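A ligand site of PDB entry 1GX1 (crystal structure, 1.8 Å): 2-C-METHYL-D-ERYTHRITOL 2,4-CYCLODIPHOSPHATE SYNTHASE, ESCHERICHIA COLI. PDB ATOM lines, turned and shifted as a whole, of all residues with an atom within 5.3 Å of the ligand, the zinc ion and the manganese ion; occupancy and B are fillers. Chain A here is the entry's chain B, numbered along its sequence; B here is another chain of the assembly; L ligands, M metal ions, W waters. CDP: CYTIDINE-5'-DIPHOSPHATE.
The zinc ion is bound by an oxygen (O2B) of the ligand, 1.7 Å away. NE2 of His 11 of chain B binds the zinc ion, 1.9 Å away. The zinc ion is bound by the side-chain carboxylate (OD2) of Asp 9 of chain B. The zinc ion is bound by ND1 of His 43 of chain B, at 2.0 Å. The zinc ion has four donor atoms within binding distance.
Merely in contact with the ligand: Ala 132, Lys 105, Lys 60 of chain B and Ile 58 of chain B. Hydrophobic or aromatic side chains that line the ligand: Ala 101, Met 106, Leu 107, Ala 132, His 11 of chain B, His 43 of chain B and Ile 58 of chain B. Of the 24 residues printed, 16 come within 4 Å of the ligand.
Within 4 Å of the manganese ion: Glu 136. The nearest printed residue that does not touch the manganese ion is His 11 of chain B (4.2 Å).
The side-chain hydroxyl (OG1) of Thr 134 sits at hydrogen-bond distance from the backbone NH (N) of Glu 136. The side-chain carboxylate (OD1) of Asp 57 of chain B lies within hydrogen-bond range of the backbone NH (N) of Gly 59 of chain B (3.0 Å). The side-chain carboxylate (OD2) of Asp 57 of chain B sits at hydrogen-bond distance from the backbone NH (N) of Ala 132, at 3.3 Å. The side-chain carboxylate of Asp 57 of chain B sits at hydrogen-bond distance from the backbone NH of Lys 60 of chain B, at 2.8 Å. N of Ala 101 is in hydrogen-bond range of O of Thr 133 (3.0 Å). N of Ile 58 of chain B is in hydrogen-bond range of OD1 of Asp 47 of chain B, 2.7 Å away.
The manganese ion is bound by O2A of the ligand (2.1 Å), water W8 (2.2 Å), O1B of the ligand (2.2 Å), water W6 (2.2 Å), OE1 of Glu 136 (2.3 Å) and water W2 (2.4 Å). The manganese ion has six donor atoms within binding distance.
N of Thr 134 lies within hydrogen-bond range of O1A of the ligand (2.8 Å). The side-chain hydroxyl (OG1) of Thr 134 sits at hydrogen-bond distance from an oxygen (O1A) of the ligand. The backbone NH (N) of Leu 107 is in hydrogen-bond range of an oxygen (O2) of the ligand (2.8 Å). OD1 of Asp 57 of chain B lies within hydrogen-bond range of O2' of the ligand (2.9 Å). The backbone carbonyl oxygen (O) of Ala 101 is in hydrogen-bond range of a nitrogen (N4) of the ligand, at 2.9 Å. N3 of the ligand lies within hydrogen-bond range of N of Met 106 (2.9 Å). The backbone carbonyl oxygen (O) of Pro 104 is in hydrogen-bond range of a nitrogen (N4) of the ligand, 2.9 Å away. O3' of the ligand lies within hydrogen-bond range of N of Gly 59 of chain B, at 3.2 Å. The side-chain hydroxyl of Thr 133 lies within hydrogen-bond range of an oxygen (O1A) of the ligand (3.3 Å).
Of the 24 residues printed, 3 come within 4 Å of the zinc ion.
Water W5 lies within hydrogen-bond range of OD2 of Asp 47 of chain B (2.7 Å), O3' of the ligand (2.8 Å) and O of Ala 132 (3.0 Å). Water W3 lies within hydrogen-bond range of the side-chain carboxylate (OD1) of Asp 9 of chain B, the side-chain hydroxyl (OG1) of Thr 133 and an oxygen (O3A) of the ligand. Water W4 lies within hydrogen-bond range of O2' of the ligand (3.0 Å) and O of Gly 59 of chain B (3.5 Å).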
ATOM      1  N   ALA A 101       5.615  -9.543 -27.246  1.00  0.00           N
ATOM      2  CA  ALA A 101       6.278 -10.332 -28.294  1.00  0.00           C
ATOM      3  C   ALA A 101       7.120 -11.445 -27.700  1.00  0.00           C
ATOM      4  O   ALA A 101       7.852 -11.243 -26.743  1.00  0.00           O
ATOM      5  CB  ALA A 101       7.169  -9.425 -29.144  1.00  0.00           C
ATOM      6  N   GLN A 102       7.017 -12.622 -28.277  1.00  0.00           N
ATOM      7  CA  GLN A 102       7.785 -13.751 -27.794  1.00  0.00           C
ATOM      8  C   GLN A 102       9.252 -13.588 -28.216  1.00  0.00           C
ATOM      9  O   GLN A 102      10.165 -14.053 -27.511  1.00  0.00           O
ATOM     10  CB  GLN A 102       7.230 -15.032 -28.471  1.00  0.00           C
ATOM     11  CG  GLN A 102       7.734 -16.309 -27.865  1.00  0.00           C
ATOM     12  CD  GLN A 102       7.386 -16.456 -26.391  1.00  0.00           C
ATOM     13  OE1 GLN A 102       6.288 -16.113 -25.965  1.00  0.00           O
ATOM     14  NE2 GLN A 102       8.324 -16.976 -25.632  1.00  0.00           N
ATOM     15  N   ALA A 103       9.410 -12.940 -29.355  1.00  0.00           N
ATOM     16  CA  ALA A 103      10.725 -12.700 -30.005  1.00  0.00           C
ATOM     17  C   ALA A 103      10.475 -11.722 -31.141  1.00  0.00           C
ATOM     18  O   ALA A 103       9.365 -11.618 -31.633  1.00  0.00           O
ATOM     19  CB  ALA A 103      11.281 -14.056 -30.562  1.00  0.00           C
ATOM     20  N   PRO A 104      11.464 -10.950 -31.574  1.00  0.00           N
ATOM     21  CA  PRO A 104      12.829 -10.970 -31.032  1.00  0.00           C
ATOM     22  C   PRO A 104      12.952 -10.259 -29.722  1.00  0.00           C
ATOM     23  O   PRO A 104      12.017  -9.600 -29.229  1.00  0.00           O
ATOM     24  CB  PRO A 104      13.625 -10.133 -32.072  1.00  0.00           C
ATOM     25  CG  PRO A 104      12.618  -9.397 -32.874  1.00  0.00           C
ATOM     26  CD  PRO A 104      11.268  -9.969 -32.644  1.00  0.00           C
ATOM     27  N   LYS A 105      14.151 -10.363 -29.155  1.00  0.00           N
ATOM     28  CA  LYS A 105      14.453  -9.670 -27.912  1.00  0.00           C
ATOM     29  C   LYS A 105      14.466  -8.155 -28.173  1.00  0.00           C
ATOM     30  O   LYS A 105      15.155  -7.657 -29.078  1.00  0.00           O
ATOM     31  CB  LYS A 105      15.797 -10.150 -27.360  1.00  0.00           C
ATOM     32  CG  LYS A 105      16.028  -9.702 -25.947  1.00  0.00           C
ATOM     33  CD  LYS A 105      15.489 -10.708 -24.928  1.00  0.00           C
ATOM     34  CE  LYS A 105      15.780 -10.180 -23.525  1.00  0.00           C
ATOM     35  NZ  LYS A 105      17.280 -10.130 -23.277  1.00  0.00           N
ATOM     36  N   MET A 106      13.691  -7.415 -27.390  1.00  0.00           N
ATOM     37  CA  MET A 106      13.522  -5.968 -27.590  1.00  0.00           C
ATOM     38  C   MET A 106      14.475  -5.136 -26.738  1.00  0.00           C
ATOM     39  O   MET A 106      14.864  -4.034 -27.139  1.00  0.00           O
ATOM     40  CB  MET A 106      12.083  -5.529 -27.226  1.00  0.00           C
ATOM     41  CG  MET A 106      10.984  -6.221 -28.019  1.00  0.00           C
ATOM     42  SD  MET A 106      11.061  -5.706 -29.889  1.00  0.00           S
ATOM     43  CE  MET A 106       9.934  -7.224 -30.605  1.00  0.00           C
ATOM     44  N   LEU A 107      14.837  -5.651 -25.568  1.00  0.00           N
ATOM     45  CA  LEU A 107      15.600  -4.841 -24.611  1.00  0.00           C
ATOM     46  C   LEU A 107      16.814  -4.078 -25.183  1.00  0.00           C
ATOM     47  O   LEU A 107      16.988  -2.900 -24.941  1.00  0.00           O
ATOM     48  CB  LEU A 107      16.014  -5.688 -23.404  1.00  0.00           C
ATOM     49  CG  LEU A 107      16.517  -4.928 -22.167  1.00  0.00           C
ATOM     50  CD1 LEU A 107      15.599  -3.724 -21.880  1.00  0.00           C
ATOM     51  CD2 LEU A 107      16.665  -5.863 -20.927  1.00  0.00           C
ATOM     52  N   PRO A 108      17.642  -4.745 -25.986  1.00  0.00           N
ATOM     53  CA  PRO A 108      18.831  -4.090 -26.535  1.00  0.00           C
ATOM     54  C   PRO A 108      18.470  -2.906 -27.412  1.00  0.00           C
ATOM     55  O   PRO A 108      19.262  -1.977 -27.596  1.00  0.00           O
ATOM     56  CB  PRO A 108      19.431  -5.180 -27.461  1.00  0.00           C
ATOM     57  CG  PRO A 108      18.927  -6.435 -26.954  1.00  0.00           C
ATOM     58  CD  PRO A 108      17.519  -6.137 -26.417  1.00  0.00           C
ATOM     59  N   ALA A 132       9.073  -4.445 -22.606  1.00  0.00           N
ATOM     60  CA  ALA A 132       8.554  -5.574 -23.385  1.00  0.00           C
ATOM     61  C   ALA A 132       8.284  -6.727 -22.460  1.00  0.00           C
ATOM     62  O   ALA A 132       8.887  -6.820 -21.344  1.00  0.00           O
ATOM     63  CB  ALA A 132       9.557  -5.976 -24.481  1.00  0.00           C
ATOM     64  N   THR A 133       7.405  -7.627 -22.899  1.00  0.00           N
ATOM     65  CA  THR A 133       7.142  -8.825 -22.177  1.00  0.00           C
ATOM     66  C   THR A 133       6.782  -9.931 -23.192  1.00  0.00           C
ATOM     67  O   THR A 133       6.341  -9.634 -24.305  1.00  0.00           O
ATOM     68  CB  THR A 133       5.992  -8.651 -21.126  1.00  0.00           C
ATOM     69  OG1 THR A 133       5.744  -9.911 -20.461  1.00  0.00           O
ATOM     70  CG2 THR A 133       4.654  -8.378 -21.804  1.00  0.00           C
ATOM     71  N   THR A 134       6.977 -11.187 -22.802  1.00  0.00           N
ATOM     72  CA  THR A 134       6.445 -12.301 -23.591  1.00  0.00           C
ATOM     73  C   THR A 134       5.125 -12.729 -22.959  1.00  0.00           C
ATOM     74  O   THR A 134       4.836 -12.317 -21.829  1.00  0.00           O
ATOM     75  CB  THR A 134       7.357 -13.573 -23.592  1.00  0.00           C
ATOM     76  OG1 THR A 134       7.335 -14.211 -22.303  1.00  0.00           O
ATOM     77  CG2 THR A 134       8.794 -13.217 -23.856  1.00  0.00           C
ATOM     78  N   THR A 135       4.391 -13.616 -23.638  1.00  0.00           N
ATOM     79  CA  THR A 135       3.214 -14.252 -23.034  1.00  0.00           C
ATOM     80  C   THR A 135       3.536 -15.725 -22.775  1.00  0.00           C
ATOM     81  O   THR A 135       2.623 -16.576 -22.718  1.00  0.00           O
ATOM     82  CB  THR A 135       1.986 -14.146 -23.908  1.00  0.00           C
ATOM     83  OG1 THR A 135       2.299 -14.691 -25.210  1.00  0.00           O
ATOM     84  CG2 THR A 135       1.624 -12.669 -24.198  1.00  0.00           C
ATOM     85  N   GLU A 136       4.814 -16.026 -22.566  1.00  0.00           N
ATOM     86  CA  GLU A 136       5.238 -17.364 -22.144  1.00  0.00           C
ATOM     87  C   GLU A 136       4.700 -18.453 -23.092  1.00  0.00           C
ATOM     88  O   GLU A 136       4.169 -19.489 -22.639  1.00  0.00           O
ATOM     89  CB  GLU A 136       4.783 -17.630 -20.720  1.00  0.00           C
ATOM     90  CG  GLU A 136       5.283 -16.569 -19.732  1.00  0.00           C
ATOM     91  CD  GLU A 136       6.781 -16.616 -19.510  1.00  0.00           C
ATOM     92  OE1 GLU A 136       7.354 -15.574 -19.089  1.00  0.00           O
ATOM     93  OE2 GLU A 136       7.383 -17.707 -19.774  1.00  0.00           O
ATOM     94  N   ASP B   9       1.450  -8.455 -17.945  1.00  0.00           N
ATOM     95  CA  ASP B   9       2.199  -9.705 -17.791  1.00  0.00           C
ATOM     96  C   ASP B   9       1.294 -10.915 -17.987  1.00  0.00           C
ATOM     97  O   ASP B   9       0.038 -10.848 -17.879  1.00  0.00           O
ATOM     98  CB  ASP B   9       2.849  -9.759 -16.409  1.00  0.00           C
ATOM     99  CG  ASP B   9       3.977 -10.769 -16.318  1.00  0.00           C
ATOM    100  OD1 ASP B   9       4.558 -11.232 -17.362  1.00  0.00           O
ATOM    101  OD2 ASP B   9       4.317 -11.147 -15.214  1.00  0.00           O
ATOM    102  N   VAL B  10       1.952 -12.030 -18.273  1.00  0.00           N
ATOM    103  CA  VAL B  10       1.292 -13.302 -18.459  1.00  0.00           C
ATOM    104  C   VAL B  10       2.191 -14.425 -17.866  1.00  0.00           C
ATOM    105  O   VAL B  10       3.423 -14.384 -18.022  1.00  0.00           O
ATOM    106  CB  VAL B  10       1.106 -13.599 -19.997  1.00  0.00           C
ATOM    107  CG1 VAL B  10       0.639 -15.047 -20.185  1.00  0.00           C
ATOM    108  CG2 VAL B  10       0.141 -12.642 -20.656  1.00  0.00           C
ATOM    109  N   HIS B  11       1.589 -15.399 -17.198  1.00  0.00           N
ATOM    110  CA  HIS B  11       2.296 -16.616 -16.841  1.00  0.00           C
ATOM    111  C   HIS B  11       1.380 -17.811 -17.123  1.00  0.00           C
ATOM    112  O   HIS B  11       0.150 -17.705 -17.082  1.00  0.00           O
ATOM    113  CB  HIS B  11       2.796 -16.603 -15.384  1.00  0.00           C
ATOM    114  CG  HIS B  11       3.977 -15.700 -15.213  1.00  0.00           C
ATOM    115  ND1 HIS B  11       5.220 -16.004 -15.707  1.00  0.00           N
ATOM    116  CD2 HIS B  11       4.047 -14.419 -14.778  1.00  0.00           C
ATOM    117  CE1 HIS B  11       6.042 -14.984 -15.497  1.00  0.00           C
ATOM    118  NE2 HIS B  11       5.346 -14.003 -14.923  1.00  0.00           N
ATOM    119  N   ASP B  39       4.037 -14.354  -9.994  1.00  0.00           N
ATOM    120  CA  ASP B  39       2.940 -13.474  -9.554  1.00  0.00           C
ATOM    121  C   ASP B  39       2.662 -12.418 -10.642  1.00  0.00           C
ATOM    122  O   ASP B  39       3.282 -11.327 -10.643  1.00  0.00           O
ATOM    123  CB  ASP B  39       3.317 -12.804  -8.231  1.00  0.00           C
ATOM    124  CG  ASP B  39       2.142 -12.113  -7.576  1.00  0.00           C
ATOM    125  OD1 ASP B  39       1.217 -11.622  -8.317  1.00  0.00           O
ATOM    126  OD2 ASP B  39       2.101 -11.997  -6.320  1.00  0.00           O
ATOM    127  N   VAL B  40       1.727 -12.718 -11.543  1.00  0.00           N
ATOM    128  CA  VAL B  40       1.523 -11.862 -12.675  1.00  0.00           C
ATOM    129  C   VAL B  40       1.043 -10.507 -12.268  1.00  0.00           C
ATOM    130  O   VAL B  40       1.360  -9.541 -12.909  1.00  0.00           O
ATOM    131  CB  VAL B  40       0.357 -12.283 -13.564  1.00  0.00           C
ATOM    132  CG1 VAL B  40       0.807 -12.653 -14.952  1.00  0.00           C
ATOM    133  CG2 VAL B  40      -0.635 -13.257 -12.862  1.00  0.00           C
ATOM    134  N   HIS B  43       4.066  -8.471 -10.960  1.00  0.00           N
ATOM    135  CA  HIS B  43       4.909  -8.115 -12.095  1.00  0.00           C
ATOM    136  C   HIS B  43       4.347  -6.975 -12.940  1.00  0.00           C
ATOM    137  O   HIS B  43       5.061  -6.016 -13.269  1.00  0.00           O
ATOM    138  CB  HIS B  43       5.136  -9.344 -12.992  1.00  0.00           C
ATOM    139  CG  HIS B  43       5.969 -10.411 -12.326  1.00  0.00           C
ATOM    140  ND1 HIS B  43       6.329 -11.580 -12.959  1.00  0.00           N
ATOM    141  CD2 HIS B  43       6.505 -10.456 -11.092  1.00  0.00           C
ATOM    142  CE1 HIS B  43       7.037 -12.320 -12.113  1.00  0.00           C
ATOM    143  NE2 HIS B  43       7.144 -11.667 -10.974  1.00  0.00           N
ATOM    144  N   ASP B  47       5.920  -3.295 -13.247  1.00  0.00           N
ATOM    145  CA  ASP B  47       6.204  -2.657 -14.545  1.00  0.00           C
ATOM    146  C   ASP B  47       5.480  -1.286 -14.730  1.00  0.00           C
ATOM    147  O   ASP B  47       6.056  -0.356 -15.319  1.00  0.00           O
ATOM    148  CB  ASP B  47       5.879  -3.566 -15.744  1.00  0.00           C
ATOM    149  CG  ASP B  47       7.061  -4.448 -16.180  1.00  0.00           C
ATOM    150  OD1 ASP B  47       8.209  -4.222 -15.699  1.00  0.00           O
ATOM    151  OD2 ASP B  47       6.926  -5.392 -17.021  1.00  0.00           O
ATOM    152  N   ASP B  57      11.838  -1.711 -17.096  1.00  0.00           N
ATOM    153  CA  ASP B  57      10.929  -2.803 -16.779  1.00  0.00           C
ATOM    154  C   ASP B  57      11.589  -3.793 -15.804  1.00  0.00           C
ATOM    155  O   ASP B  57      12.771  -3.654 -15.528  1.00  0.00           O
ATOM    156  CB  ASP B  57      10.368  -3.451 -18.071  1.00  0.00           C
ATOM    157  CG  ASP B  57      11.445  -4.175 -18.954  1.00  0.00           C
ATOM    158  OD1 ASP B  57      12.380  -4.802 -18.402  1.00  0.00           O
ATOM    159  OD2 ASP B  57      11.404  -4.198 -20.221  1.00  0.00           O
ATOM    160  N   ILE B  58      10.837  -4.743 -15.241  1.00  0.00           N
ATOM    161  CA  ILE B  58      11.435  -5.668 -14.265  1.00  0.00           C
ATOM    162  C   ILE B  58      12.624  -6.452 -14.829  1.00  0.00           C
ATOM    163  O   ILE B  58      13.554  -6.801 -14.089  1.00  0.00           O
ATOM    164  CB  ILE B  58      10.413  -6.675 -13.710  1.00  0.00           C
ATOM    165  CG1 ILE B  58       9.734  -7.480 -14.837  1.00  0.00           C
ATOM    166  CG2 ILE B  58       9.435  -6.004 -12.861  1.00  0.00           C
ATOM    167  CD1 ILE B  58       8.481  -8.186 -14.320  1.00  0.00           C
ATOM    168  N   GLY B  59      12.599  -6.713 -16.127  1.00  0.00           N
ATOM    169  CA  GLY B  59      13.680  -7.443 -16.765  1.00  0.00           C
ATOM    170  C   GLY B  59      14.934  -6.589 -16.864  1.00  0.00           C
ATOM    171  O   GLY B  59      16.049  -7.086 -16.801  1.00  0.00           O
ATOM    172  N   LYS B  60      14.794  -5.286 -17.009  1.00  0.00           N
ATOM    173  CA  LYS B  60      15.988  -4.463 -17.032  1.00  0.00           C
ATOM    174  C   LYS B  60      16.619  -4.389 -15.620  1.00  0.00           C
ATOM    175  O   LYS B  60      17.842  -4.479 -15.470  1.00  0.00           O
ATOM    176  CB  LYS B  60      15.630  -3.074 -17.498  1.00  0.00           C
ATOM    177  CG  LYS B  60      16.829  -2.164 -17.753  1.00  0.00           C
ATOM    178  CD  LYS B  60      16.319  -0.760 -17.944  1.00  0.00           C
ATOM    179  CE  LYS B  60      17.428   0.159 -18.446  1.00  0.00           C
ATOM    180  NZ  LYS B  60      18.469   0.403 -17.393  1.00  0.00           N
HETATM  181  O3B CDP L   1       9.820 -11.780 -15.898  1.00  0.00           O
HETATM  182  PB  CDP L   1       8.526 -12.308 -16.662  1.00  0.00           P
HETATM  183  O1B CDP L   1       8.645 -13.775 -16.643  1.00  0.00           O
HETATM  184  O2B CDP L   1       7.196 -11.730 -15.917  1.00  0.00           O
HETATM  185  O3A CDP L   1       8.852 -11.741 -18.150  1.00  0.00           O
HETATM  186  PA  CDP L   1       9.238 -12.394 -19.586  1.00  0.00           P
HETATM  187  O1A CDP L   1       8.105 -12.278 -20.536  1.00  0.00           O
HETATM  188  O2A CDP L   1       9.843 -13.793 -19.458  1.00  0.00           O
HETATM  189  O5' CDP L   1      10.296 -11.303 -20.080  1.00  0.00           O
HETATM  190  C5' CDP L   1      11.456 -11.017 -19.333  1.00  0.00           C
HETATM  191  C4' CDP L   1      12.213  -9.793 -19.825  1.00  0.00           C
HETATM  192  O4' CDP L   1      12.632  -9.945 -21.161  1.00  0.00           O
HETATM  193  C3' CDP L   1      11.289  -8.574 -19.878  1.00  0.00           C
HETATM  194  O3' CDP L   1      11.045  -8.045 -18.564  1.00  0.00           O
HETATM  195  C2' CDP L   1      12.013  -7.678 -20.850  1.00  0.00           C
HETATM  196  O2' CDP L   1      13.020  -7.050 -20.081  1.00  0.00           O
HETATM  197  C1' CDP L   1      12.632  -8.714 -21.828  1.00  0.00           C
HETATM  198  N1  CDP L   1      11.913  -8.934 -23.100  1.00  0.00           N
HETATM  199  C2  CDP L   1      12.476  -8.470 -24.250  1.00  0.00           C
HETATM  200  O2  CDP L   1      13.432  -7.664 -24.178  1.00  0.00           O
HETATM  201  N3  CDP L   1      11.991  -8.865 -25.476  1.00  0.00           N
HETATM  202  C4  CDP L   1      10.788  -9.496 -25.594  1.00  0.00           C
HETATM  203  N4  CDP L   1      10.308  -9.692 -26.827  1.00  0.00           N
HETATM  204  C5  CDP L   1      10.106  -9.874 -24.437  1.00  0.00           C
HETATM  205  C6  CDP L   1      10.700  -9.611 -23.185  1.00  0.00           C
HETATM  206 ZN    ZN M   1       5.941 -12.167 -14.808  1.00  0.00          ZN
HETATM  207 MN    MN M   2       9.422 -15.289 -18.033  1.00  0.00          MN
HETATM  208  O   HOH W   1       9.393 -15.180 -13.785  1.00  0.00           O
HETATM  209  O   HOH W   2       8.785 -16.955 -16.484  1.00  0.00           O
HETATM  210  O   HOH W   3       6.834  -9.416 -17.681  1.00  0.00           O
HETATM  211  O   HOH W   4      15.415  -8.756 -19.796  1.00  0.00           O
HETATM  212  O   HOH W   5       8.453  -7.119 -18.392  1.00  0.00           O
HETATM  213  O   HOH W   6      10.078 -16.750 -19.545  1.00  0.00           O
HETATM  214  O   HOH W   7       5.817 -13.258 -18.968  1.00  0.00           O
HETATM  215  O   HOH W   8      11.513 -15.317 -17.417  1.00  0.00           O
